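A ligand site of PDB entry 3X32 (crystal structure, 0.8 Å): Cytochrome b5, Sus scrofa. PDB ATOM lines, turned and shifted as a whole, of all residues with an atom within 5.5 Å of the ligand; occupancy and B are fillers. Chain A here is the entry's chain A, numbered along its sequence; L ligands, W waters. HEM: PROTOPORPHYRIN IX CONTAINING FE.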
ATOM      1  N   LEU A  28     -21.806  18.897 -17.972  1.00  0.00           N
ATOM      2  CA  LEU A  28     -22.764  17.811 -18.211  1.00  0.00           C
ATOM      3  C   LEU A  28     -23.939  18.062 -17.261  1.00  0.00           C
ATOM      4  O   LEU A  28     -23.882  18.934 -16.363  1.00  0.00           O
ATOM      5  CB  LEU A  28     -22.122  16.429 -18.172  1.00  0.00           C
ATOM      6  CG  LEU A  28     -21.329  16.030 -16.944  1.00  0.00           C
ATOM      7  CD1 LEU A  28     -22.208  15.822 -15.711  1.00  0.00           C
ATOM      8  CD2 LEU A  28     -20.535  14.769 -17.232  1.00  0.00           C
ATOM      9  N   LEU A  30     -26.579  16.200 -14.491  1.00  0.00           N
ATOM     10  CA  LEU A  30     -26.929  15.063 -13.625  1.00  0.00           C
ATOM     11  C   LEU A  30     -28.174  15.474 -12.876  1.00  0.00           C
ATOM     12  O   LEU A  30     -28.169  16.512 -12.176  1.00  0.00           O
ATOM     13  CB  LEU A  30     -25.846  14.715 -12.632  1.00  0.00           C
ATOM     14  CG  LEU A  30     -24.483  14.450 -13.177  1.00  0.00           C
ATOM     15  CD1 LEU A  30     -23.432  14.418 -12.036  1.00  0.00           C
ATOM     16  CD2 LEU A  30     -24.433  13.173 -13.993  1.00  0.00           C
ATOM     17  N   TYR A  35     -23.236  20.765 -14.286  1.00  0.00           N
ATOM     18  CA  TYR A  35     -21.974  20.661 -13.654  1.00  0.00           C
ATOM     19  C   TYR A  35     -20.880  21.097 -14.630  1.00  0.00           C
ATOM     20  O   TYR A  35     -20.807  20.613 -15.756  1.00  0.00           O
ATOM     21  CB  TYR A  35     -21.674  19.179 -13.276  1.00  0.00           C
ATOM     22  CG  TYR A  35     -22.653  18.648 -12.251  1.00  0.00           C
ATOM     23  CD1 TYR A  35     -23.962  18.334 -12.610  1.00  0.00           C
ATOM     24  CD2 TYR A  35     -22.292  18.503 -10.919  1.00  0.00           C
ATOM     25  CE1 TYR A  35     -24.868  17.906 -11.632  1.00  0.00           C
ATOM     26  CE2 TYR A  35     -23.179  18.042  -9.959  1.00  0.00           C
ATOM     27  CZ  TYR A  35     -24.484  17.778 -10.340  1.00  0.00           C
ATOM     28  OH  TYR A  35     -25.412  17.391  -9.411  1.00  0.00           O
ATOM     29  N   LEU A  37     -17.320  20.576 -15.366  1.00  0.00           N
ATOM     30  CA  LEU A  37     -16.284  19.592 -15.079  1.00  0.00           C
ATOM     31  C   LEU A  37     -14.992  19.865 -15.877  1.00  0.00           C
ATOM     32  O   LEU A  37     -14.122  18.999 -15.950  1.00  0.00           O
ATOM     33  CB  LEU A  37     -16.752  18.172 -15.299  1.00  0.00           C
ATOM     34  CG  LEU A  37     -18.007  17.791 -14.494  1.00  0.00           C
ATOM     35  CD1 LEU A  37     -18.283  16.305 -14.670  1.00  0.00           C
ATOM     36  CD2 LEU A  37     -17.865  18.133 -13.029  1.00  0.00           C
ATOM     37  N   PHE A  40     -12.229  19.471 -13.415  1.00  0.00           N
ATOM     38  CA  PHE A  40     -12.367  18.199 -12.676  1.00  0.00           C
ATOM     39  C   PHE A  40     -11.968  17.022 -13.507  1.00  0.00           C
ATOM     40  O   PHE A  40     -11.467  16.027 -12.983  1.00  0.00           O
ATOM     41  CB  PHE A  40     -13.787  18.052 -12.165  1.00  0.00           C
ATOM     42  CG  PHE A  40     -13.949  16.742 -11.445  1.00  0.00           C
ATOM     43  CD1 PHE A  40     -13.281  16.483 -10.258  1.00  0.00           C
ATOM     44  CD2 PHE A  40     -14.773  15.698 -11.956  1.00  0.00           C
ATOM     45  CE1 PHE A  40     -13.404  15.269  -9.626  1.00  0.00           C
ATOM     46  CE2 PHE A  40     -14.900  14.510 -11.310  1.00  0.00           C
ATOM     47  CZ  PHE A  40     -14.228  14.277 -10.150  1.00  0.00           C
ATOM     48  N   HIS A  44     -10.508  13.319 -12.105  1.00  0.00           N
ATOM     49  CA  HIS A  44     -11.544  12.335 -11.835  1.00  0.00           C
ATOM     50  C   HIS A  44     -10.945  10.930 -11.750  1.00  0.00           C
ATOM     51  O   HIS A  44     -10.260  10.471 -12.671  1.00  0.00           O
ATOM     52  CB  HIS A  44     -12.488  12.353 -13.036  1.00  0.00           C
ATOM     53  CG  HIS A  44     -13.591  11.345 -12.942  1.00  0.00           C
ATOM     54  ND1 HIS A  44     -13.938  10.506 -13.992  1.00  0.00           N
ATOM     55  CD2 HIS A  44     -14.488  11.054 -11.942  1.00  0.00           C
ATOM     56  CE1 HIS A  44     -14.988   9.772 -13.616  1.00  0.00           C
ATOM     57  NE2 HIS A  44     -15.353  10.073 -12.394  1.00  0.00           N
ATOM     58  N   PRO A  45     -11.232  10.165 -10.656  1.00  0.00           N
ATOM     59  CA  PRO A  45     -10.654   8.824 -10.561  1.00  0.00           C
ATOM     60  C   PRO A  45     -11.064   7.847 -11.639  1.00  0.00           C
ATOM     61  O   PRO A  45     -10.275   6.928 -11.982  1.00  0.00           O
ATOM     62  CB  PRO A  45     -11.127   8.316  -9.192  1.00  0.00           C
ATOM     63  CG  PRO A  45     -11.184   9.593  -8.399  1.00  0.00           C
ATOM     64  CD  PRO A  45     -11.791  10.673  -9.342  1.00  0.00           C
ATOM     65  N   GLY A  46     -12.225   8.059 -12.245  1.00  0.00           N
ATOM     66  CA  GLY A  46     -12.655   7.233 -13.355  1.00  0.00           C
ATOM     67  C   GLY A  46     -12.082   7.593 -14.710  1.00  0.00           C
ATOM     68  O   GLY A  46     -12.436   6.965 -15.707  1.00  0.00           O
ATOM     69  N   VAL A  50     -14.467   9.122 -19.934  1.00  0.00           N
ATOM     70  CA  VAL A  50     -15.863   8.835 -19.670  1.00  0.00           C
ATOM     71  C   VAL A  50     -16.675  10.124 -19.534  1.00  0.00           C
ATOM     72  O   VAL A  50     -17.851  10.165 -19.877  1.00  0.00           O
ATOM     73  CB  VAL A  50     -16.075   7.929 -18.454  1.00  0.00           C
ATOM     74  CG1 VAL A  50     -15.544   6.538 -18.748  1.00  0.00           C
ATOM     75  CG2 VAL A  50     -15.543   8.482 -17.147  1.00  0.00           C
ATOM     76  N   LEU A  51     -15.939  11.107 -18.939  1.00  0.00           N
ATOM     77  CA  LEU A  51     -16.576  12.407 -18.805  1.00  0.00           C
ATOM     78  C   LEU A  51     -16.641  13.143 -20.151  1.00  0.00           C
ATOM     79  O   LEU A  51     -17.708  13.710 -20.483  1.00  0.00           O
ATOM     80  CB  LEU A  51     -15.874  13.251 -17.755  1.00  0.00           C
ATOM     81  CG  LEU A  51     -15.801  12.631 -16.382  1.00  0.00           C
ATOM     82  CD1 LEU A  51     -15.068  13.567 -15.421  1.00  0.00           C
ATOM     83  CD2 LEU A  51     -17.168  12.259 -15.830  1.00  0.00           C
ATOM     84  N   GLN A  54     -19.531  12.335 -22.340  1.00  0.00           N
ATOM     85  CA  GLN A  54     -20.810  12.847 -21.896  1.00  0.00           C
ATOM     86  C   GLN A  54     -20.967  14.366 -22.055  1.00  0.00           C
ATOM     87  O   GLN A  54     -22.043  14.902 -21.791  1.00  0.00           O
ATOM     88  CB  GLN A  54     -21.025  12.507 -20.413  1.00  0.00           C
ATOM     89  CG  GLN A  54     -21.045  11.012 -20.152  1.00  0.00           C
ATOM     90  CD  GLN A  54     -22.173  10.335 -20.914  1.00  0.00           C
ATOM     91  OE1 GLN A  54     -23.284  10.897 -21.000  1.00  0.00           O
ATOM     92  NE2 GLN A  54     -21.890   9.159 -21.436  1.00  0.00           N
ATOM     93  N   ALA A  59     -25.778  12.846 -18.160  1.00  0.00           N
ATOM     94  CA  ALA A  59     -25.005  11.696 -17.794  1.00  0.00           C
ATOM     95  C   ALA A  59     -25.539  11.024 -16.521  1.00  0.00           C
ATOM     96  O   ALA A  59     -24.821  10.290 -15.835  1.00  0.00           O
ATOM     97  CB  ALA A  59     -23.538  12.031 -17.606  1.00  0.00           C
ATOM     98  N   ASN A  62     -25.304   7.166 -16.300  1.00  0.00           N
ATOM     99  CA  ASN A  62     -23.946   6.700 -16.160  1.00  0.00           C
ATOM    100  C   ASN A  62     -23.470   6.897 -14.738  1.00  0.00           C
ATOM    101  O   ASN A  62     -22.827   6.022 -14.137  1.00  0.00           O
ATOM    102  CB  ASN A  62     -22.967   7.435 -17.096  1.00  0.00           C
ATOM    103  CG  ASN A  62     -23.452   7.513 -18.504  1.00  0.00           C
ATOM    104  OD1 ASN A  62     -24.312   8.339 -18.730  1.00  0.00           O
ATOM    105  ND2 ASN A  62     -22.962   6.716 -19.390  1.00  0.00           N
ATOM    106  N   PHE A  63     -23.752   8.089 -14.145  1.00  0.00           N
ATOM    107  CA  PHE A  63     -23.303   8.408 -12.826  1.00  0.00           C
ATOM    108  C   PHE A  63     -23.868   7.403 -11.802  1.00  0.00           C
ATOM    109  O   PHE A  63     -23.143   6.907 -10.915  1.00  0.00           O
ATOM    110  CB  PHE A  63     -23.692   9.832 -12.474  1.00  0.00           C
ATOM    111  CG  PHE A  63     -23.270  10.261 -11.106  1.00  0.00           C
ATOM    112  CD1 PHE A  63     -21.999  10.770 -10.915  1.00  0.00           C
ATOM    113  CD2 PHE A  63     -24.081  10.142  -9.981  1.00  0.00           C
ATOM    114  CE1 PHE A  63     -21.525  11.169  -9.684  1.00  0.00           C
ATOM    115  CE2 PHE A  63     -23.595  10.536  -8.745  1.00  0.00           C
ATOM    116  CZ  PHE A  63     -22.350  11.021  -8.589  1.00  0.00           C
ATOM    117  N   VAL A  66     -22.523   3.590 -12.098  1.00  0.00           N
ATOM    118  CA  VAL A  66     -21.190   3.299 -11.613  1.00  0.00           C
ATOM    119  C   VAL A  66     -21.198   2.845 -10.167  1.00  0.00           C
ATOM    120  O   VAL A  66     -20.386   2.018  -9.740  1.00  0.00           O
ATOM    121  CB  VAL A  66     -20.293   4.585 -11.721  1.00  0.00           C
ATOM    122  CG1 VAL A  66     -19.038   4.544 -10.913  1.00  0.00           C
ATOM    123  CG2 VAL A  66     -19.974   4.733 -13.220  1.00  0.00           C
ATOM    124  N   GLY A  67     -22.123   3.414  -9.369  1.00  0.00           N
ATOM    125  CA  GLY A  67     -22.077   3.270  -7.973  1.00  0.00           C
ATOM    126  C   GLY A  67     -21.148   4.219  -7.309  1.00  0.00           C
ATOM    127  O   GLY A  67     -20.288   3.855  -6.456  1.00  0.00           O
ATOM    128  N   HIS A  68     -21.219   5.499  -7.619  1.00  0.00           N
ATOM    129  CA  HIS A  68     -20.439   6.532  -6.969  1.00  0.00           C
ATOM    130  C   HIS A  68     -20.724   6.560  -5.493  1.00  0.00           C
ATOM    131  O   HIS A  68     -21.842   6.522  -5.012  1.00  0.00           O
ATOM    132  CB  HIS A  68     -20.736   7.892  -7.585  1.00  0.00           C
ATOM    133  CG  HIS A  68     -20.009   8.112  -8.868  1.00  0.00           C
ATOM    134  ND1 HIS A  68     -20.527   7.826 -10.087  1.00  0.00           N
ATOM    135  CD2 HIS A  68     -18.762   8.581  -9.094  1.00  0.00           C
ATOM    136  CE1 HIS A  68     -19.641   8.148 -10.991  1.00  0.00           C
ATOM    137  NE2 HIS A  68     -18.509   8.596 -10.451  1.00  0.00           N
ATOM    138  N   SER A  69     -19.654   6.697  -4.743  1.00  0.00           N
ATOM    139  CA  SER A  69     -19.733   6.820  -3.292  1.00  0.00           C
ATOM    140  C   SER A  69     -20.481   8.071  -2.868  1.00  0.00           C
ATOM    141  O   SER A  69     -20.577   9.055  -3.607  1.00  0.00           O
ATOM    142  CB  SER A  69     -18.333   6.835  -2.733  1.00  0.00           C
ATOM    143  OG  SER A  69     -17.643   8.033  -3.067  1.00  0.00           O
ATOM    144  N   ASP A  71     -19.107  10.025  -0.844  1.00  0.00           N
ATOM    145  CA  ASP A  71     -18.046  11.003  -0.943  1.00  0.00           C
ATOM    146  C   ASP A  71     -18.039  11.656  -2.342  1.00  0.00           C
ATOM    147  O   ASP A  71     -17.894  12.877  -2.463  1.00  0.00           O
ATOM    148  CB  ASP A  71     -16.676  10.317  -0.670  1.00  0.00           C
ATOM    149  CG  ASP A  71     -16.487   9.798   0.725  1.00  0.00           C
ATOM    150  OD1 ASP A  71     -17.233  10.420   1.629  1.00  0.00           O
ATOM    151  OD2 ASP A  71     -15.541   9.040   0.982  1.00  0.00           O
ATOM    152  N   ALA A  72     -18.135  10.842  -3.352  1.00  0.00           N
ATOM    153  CA  ALA A  72     -18.163  11.360  -4.707  1.00  0.00           C
ATOM    154  C   ALA A  72     -19.406  12.266  -4.953  1.00  0.00           C
ATOM    155  O   ALA A  72     -19.318  13.282  -5.622  1.00  0.00           O
ATOM    156  CB  ALA A  72     -18.146  10.229  -5.710  1.00  0.00           C
ATOM    157  N   LEU A  75     -18.707  15.544  -3.362  1.00  0.00           N
ATOM    158  CA  LEU A  75     -17.740  16.276  -4.171  1.00  0.00           C
ATOM    159  C   LEU A  75     -18.439  16.882  -5.401  1.00  0.00           C
ATOM    160  O   LEU A  75     -18.142  18.025  -5.832  1.00  0.00           O
ATOM    161  CB  LEU A  75     -16.620  15.367  -4.565  1.00  0.00           C
ATOM    162  CG  LEU A  75     -15.536  15.978  -5.459  1.00  0.00           C
ATOM    163  CD1 LEU A  75     -14.859  17.202  -4.856  1.00  0.00           C
ATOM    164  CD2 LEU A  75     -14.555  14.900  -5.821  1.00  0.00           C
ATOM    165  N   SER A  76     -19.359  16.134  -6.026  1.00  0.00           N
ATOM    166  CA  SER A  76     -19.989  16.619  -7.258  1.00  0.00           C
ATOM    167  C   SER A  76     -20.675  17.954  -7.072  1.00  0.00           C
ATOM    168  O   SER A  76     -20.773  18.749  -7.980  1.00  0.00           O
ATOM    169  CB  SER A  76     -20.952  15.552  -7.805  1.00  0.00           C
ATOM    170  OG  SER A  76     -22.186  15.469  -7.079  1.00  0.00           O
ATOM    171  N   PHE A  79     -19.290  21.398  -8.174  1.00  0.00           N
ATOM    172  CA  PHE A  79     -19.216  21.762  -9.566  1.00  0.00           C
ATOM    173  C   PHE A  79     -20.505  22.238 -10.149  1.00  0.00           C
ATOM    174  O   PHE A  79     -20.585  22.565 -11.354  1.00  0.00           O
ATOM    175  CB  PHE A  79     -18.678  20.579 -10.405  1.00  0.00           C
ATOM    176  CG  PHE A  79     -17.385  20.048  -9.882  1.00  0.00           C
ATOM    177  CD1 PHE A  79     -16.219  20.782  -9.985  1.00  0.00           C
ATOM    178  CD2 PHE A  79     -17.307  18.836  -9.307  1.00  0.00           C
ATOM    179  CE1 PHE A  79     -15.065  20.269  -9.477  1.00  0.00           C
ATOM    180  CE2 PHE A  79     -16.173  18.293  -8.798  1.00  0.00           C
ATOM    181  CZ  PHE A  79     -15.021  19.049  -8.824  1.00  0.00           C
HETATM  182  CHA HEM L   1     -14.994   6.880 -10.009  1.00  0.00           C
HETATM  183  CHB HEM L   1     -16.193  11.374  -8.750  1.00  0.00           C
HETATM  184  CHC HEM L   1     -19.015  11.700 -12.613  1.00  0.00           C
HETATM  185  CHD HEM L   1     -17.520   7.358 -14.086  1.00  0.00           C
HETATM  186  C1A HEM L   1     -15.155   8.023  -9.279  1.00  0.00           C
HETATM  187  C2A HEM L   1     -14.604   8.274  -7.977  1.00  0.00           C
HETATM  188  C3A HEM L   1     -14.844   9.585  -7.658  1.00  0.00           C
HETATM  189  C4A HEM L   1     -15.647  10.079  -8.773  1.00  0.00           C
HETATM  190  CMA HEM L   1     -14.433  10.351  -6.474  1.00  0.00           C
HETATM  191  CAA HEM L   1     -13.922   7.237  -7.118  1.00  0.00           C
HETATM  192  CBA HEM L   1     -14.910   6.193  -6.603  1.00  0.00           C
HETATM  193  CGA HEM L   1     -16.058   6.685  -5.801  1.00  0.00           C
HETATM  194  O1A HEM L   1     -15.882   7.627  -4.992  1.00  0.00           O
HETATM  195  O2A HEM L   1     -17.171   6.142  -5.977  1.00  0.00           O
HETATM  196  C1B HEM L   1     -17.034  11.857  -9.702  1.00  0.00           C
HETATM  197  C2B HEM L   1     -17.676  13.157  -9.656  1.00  0.00           C
HETATM  198  C3B HEM L   1     -18.486  13.236 -10.713  1.00  0.00           C
HETATM  199  C4B HEM L   1     -18.345  12.000 -11.458  1.00  0.00           C
HETATM  200  CMB HEM L   1     -17.479  14.143  -8.540  1.00  0.00           C
HETATM  201  CAB HEM L   1     -19.463  14.323 -11.094  1.00  0.00           C
HETATM  202  CBB HEM L   1     -19.267  15.551 -10.975  1.00  0.00           C
HETATM  203  C1C HEM L   1     -18.890  10.530 -13.315  1.00  0.00           C
HETATM  204  C2C HEM L   1     -19.610  10.244 -14.532  1.00  0.00           C
HETATM  205  C3C HEM L   1     -19.175   9.028 -14.986  1.00  0.00           C
HETATM  206  C4C HEM L   1     -18.209   8.580 -14.014  1.00  0.00           C
HETATM  207  CMC HEM L   1     -20.723  11.173 -15.098  1.00  0.00           C
HETATM  208  CAC HEM L   1     -19.525   8.293 -16.213  1.00  0.00           C
HETATM  209  CBC HEM L   1     -19.855   8.928 -17.335  1.00  0.00           C
HETATM  210  C1D HEM L   1     -16.663   6.855 -13.114  1.00  0.00           C
HETATM  211  C2D HEM L   1     -15.972   5.591 -13.207  1.00  0.00           C
HETATM  212  C3D HEM L   1     -15.239   5.470 -12.057  1.00  0.00           C
HETATM  213  C4D HEM L   1     -15.505   6.624 -11.276  1.00  0.00           C
HETATM  214  CMD HEM L   1     -16.051   4.659 -14.366  1.00  0.00           C
HETATM  215  CAD HEM L   1     -14.281   4.352 -11.738  1.00  0.00           C
HETATM  216  CBD HEM L   1     -14.907   3.099 -11.134  1.00  0.00           C
HETATM  217  CGD HEM L   1     -15.339   3.215  -9.693  1.00  0.00           C
HETATM  218  O1D HEM L   1     -14.582   3.782  -8.890  1.00  0.00           O
HETATM  219  O2D HEM L   1     -16.429   2.677  -9.358  1.00  0.00           O
HETATM  220  NA  HEM L   1     -15.813   9.170  -9.717  1.00  0.00           N
HETATM  221  NB  HEM L   1     -17.446  11.168 -10.831  1.00  0.00           N
HETATM  222  NC  HEM L   1     -18.036   9.476 -13.022  1.00  0.00           N
HETATM  223  ND  HEM L   1     -16.366   7.518 -11.961  1.00  0.00           N
HETATM  224 FE   HEM L   1     -16.920   9.323 -11.390  1.00  0.00          FE
HETATM  225  O   HOH W   1     -14.661  11.658  -3.406  1.00  0.00           O
HETATM  226  O   HOH W   2     -19.328   4.986 -16.733  1.00  0.00           O
HETATM  227  O   HOH W   3     -14.054   8.756  -3.374  1.00  0.00           O
HETATM  228  O   HOH W   4     -18.035   0.936 -10.689  1.00  0.00           O
HETATM  229  O   HOH W   5     -12.714   3.640  -6.413  1.00  0.00           O
HETATM  230  O   HOH W   6     -11.848   3.681  -9.331  1.00  0.00           O
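A ring nitrogen (NE2) of His 68 binds an iron atom (FE) of the ligand (2.0 Å).
OG of Ser 69 lies within hydrogen-bond range of O1A of the ligand (2.6 Å).
O2A of the ligand sits at hydrogen-bond distance from N of Ser 69 (2.8 Å).
FE of the ligand is bound by NE2 of His 44.
Water W4 bridges an oxygen (O2D) of the ligand and the backbone carbonyl oxygen of Val 66.
CD2 of Leu 37 touches CBB of the ligand, at 3.6 Å.
Phe 40 touches the ligand.
Pro 45 touches the ligand.
Gly 46 touches the ligand (CA to C3D, 3.4 Å).
O of Val 50 touches CBC of the ligand (3.5 Å).
CD2 of Leu 51 touches C2C of the ligand, 3.4 Å away.
Gln 54 touches the ligand (CG to CBC, 3.7 Å).
CB of Ala 59 touches CMC of the ligand, 3.9 Å away.
Asn 62 touches the ligand.
Phe 63 touches the ligand (CD1 to CHC, 3.6 Å).
Val 66 touches the ligand (CG1 to O2D, 3.6 Å).
Gly 67 touches the ligand.
Ala 72 touches the ligand.
Ser 76 touches the ligand.
Hydrophobic or aromatic side chains within 4 Å of the ligand: Leu 37, Phe 40, His 44, Pro 45, Val 50, Leu 51, Ala 59, Phe 63, Val 66, His 68 and Ala 72.
17 residues have an atom within 4 Å of the ligand: Leu 37, Phe 40, His 44, Pro 45, Gly 46, Val 50, Leu 51, Gln 54, Ala 59, Asn 62, Phe 63, Val 66, Gly 67, His 68, Ser 69, Ala 72 and Ser 76.
The backbone NH of Ala 72 sits at hydrogen-bond distance from the side-chain hydroxyl of Ser 69 (2.9 Å).
N of Asp 71 sits close to OG of Ser 69, 3.3 Å away.
The backbone NH (N) of Gly 46 sits close to a ring nitrogen (ND1) of His 44.
NE2 of Gln 54 sits close to ND2 of Asn 62 (3.4 Å).
A ring nitrogen (ND1) of His 68 lies within hydrogen-bond range of the backbone carbonyl oxygen (O) of Phe 63.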
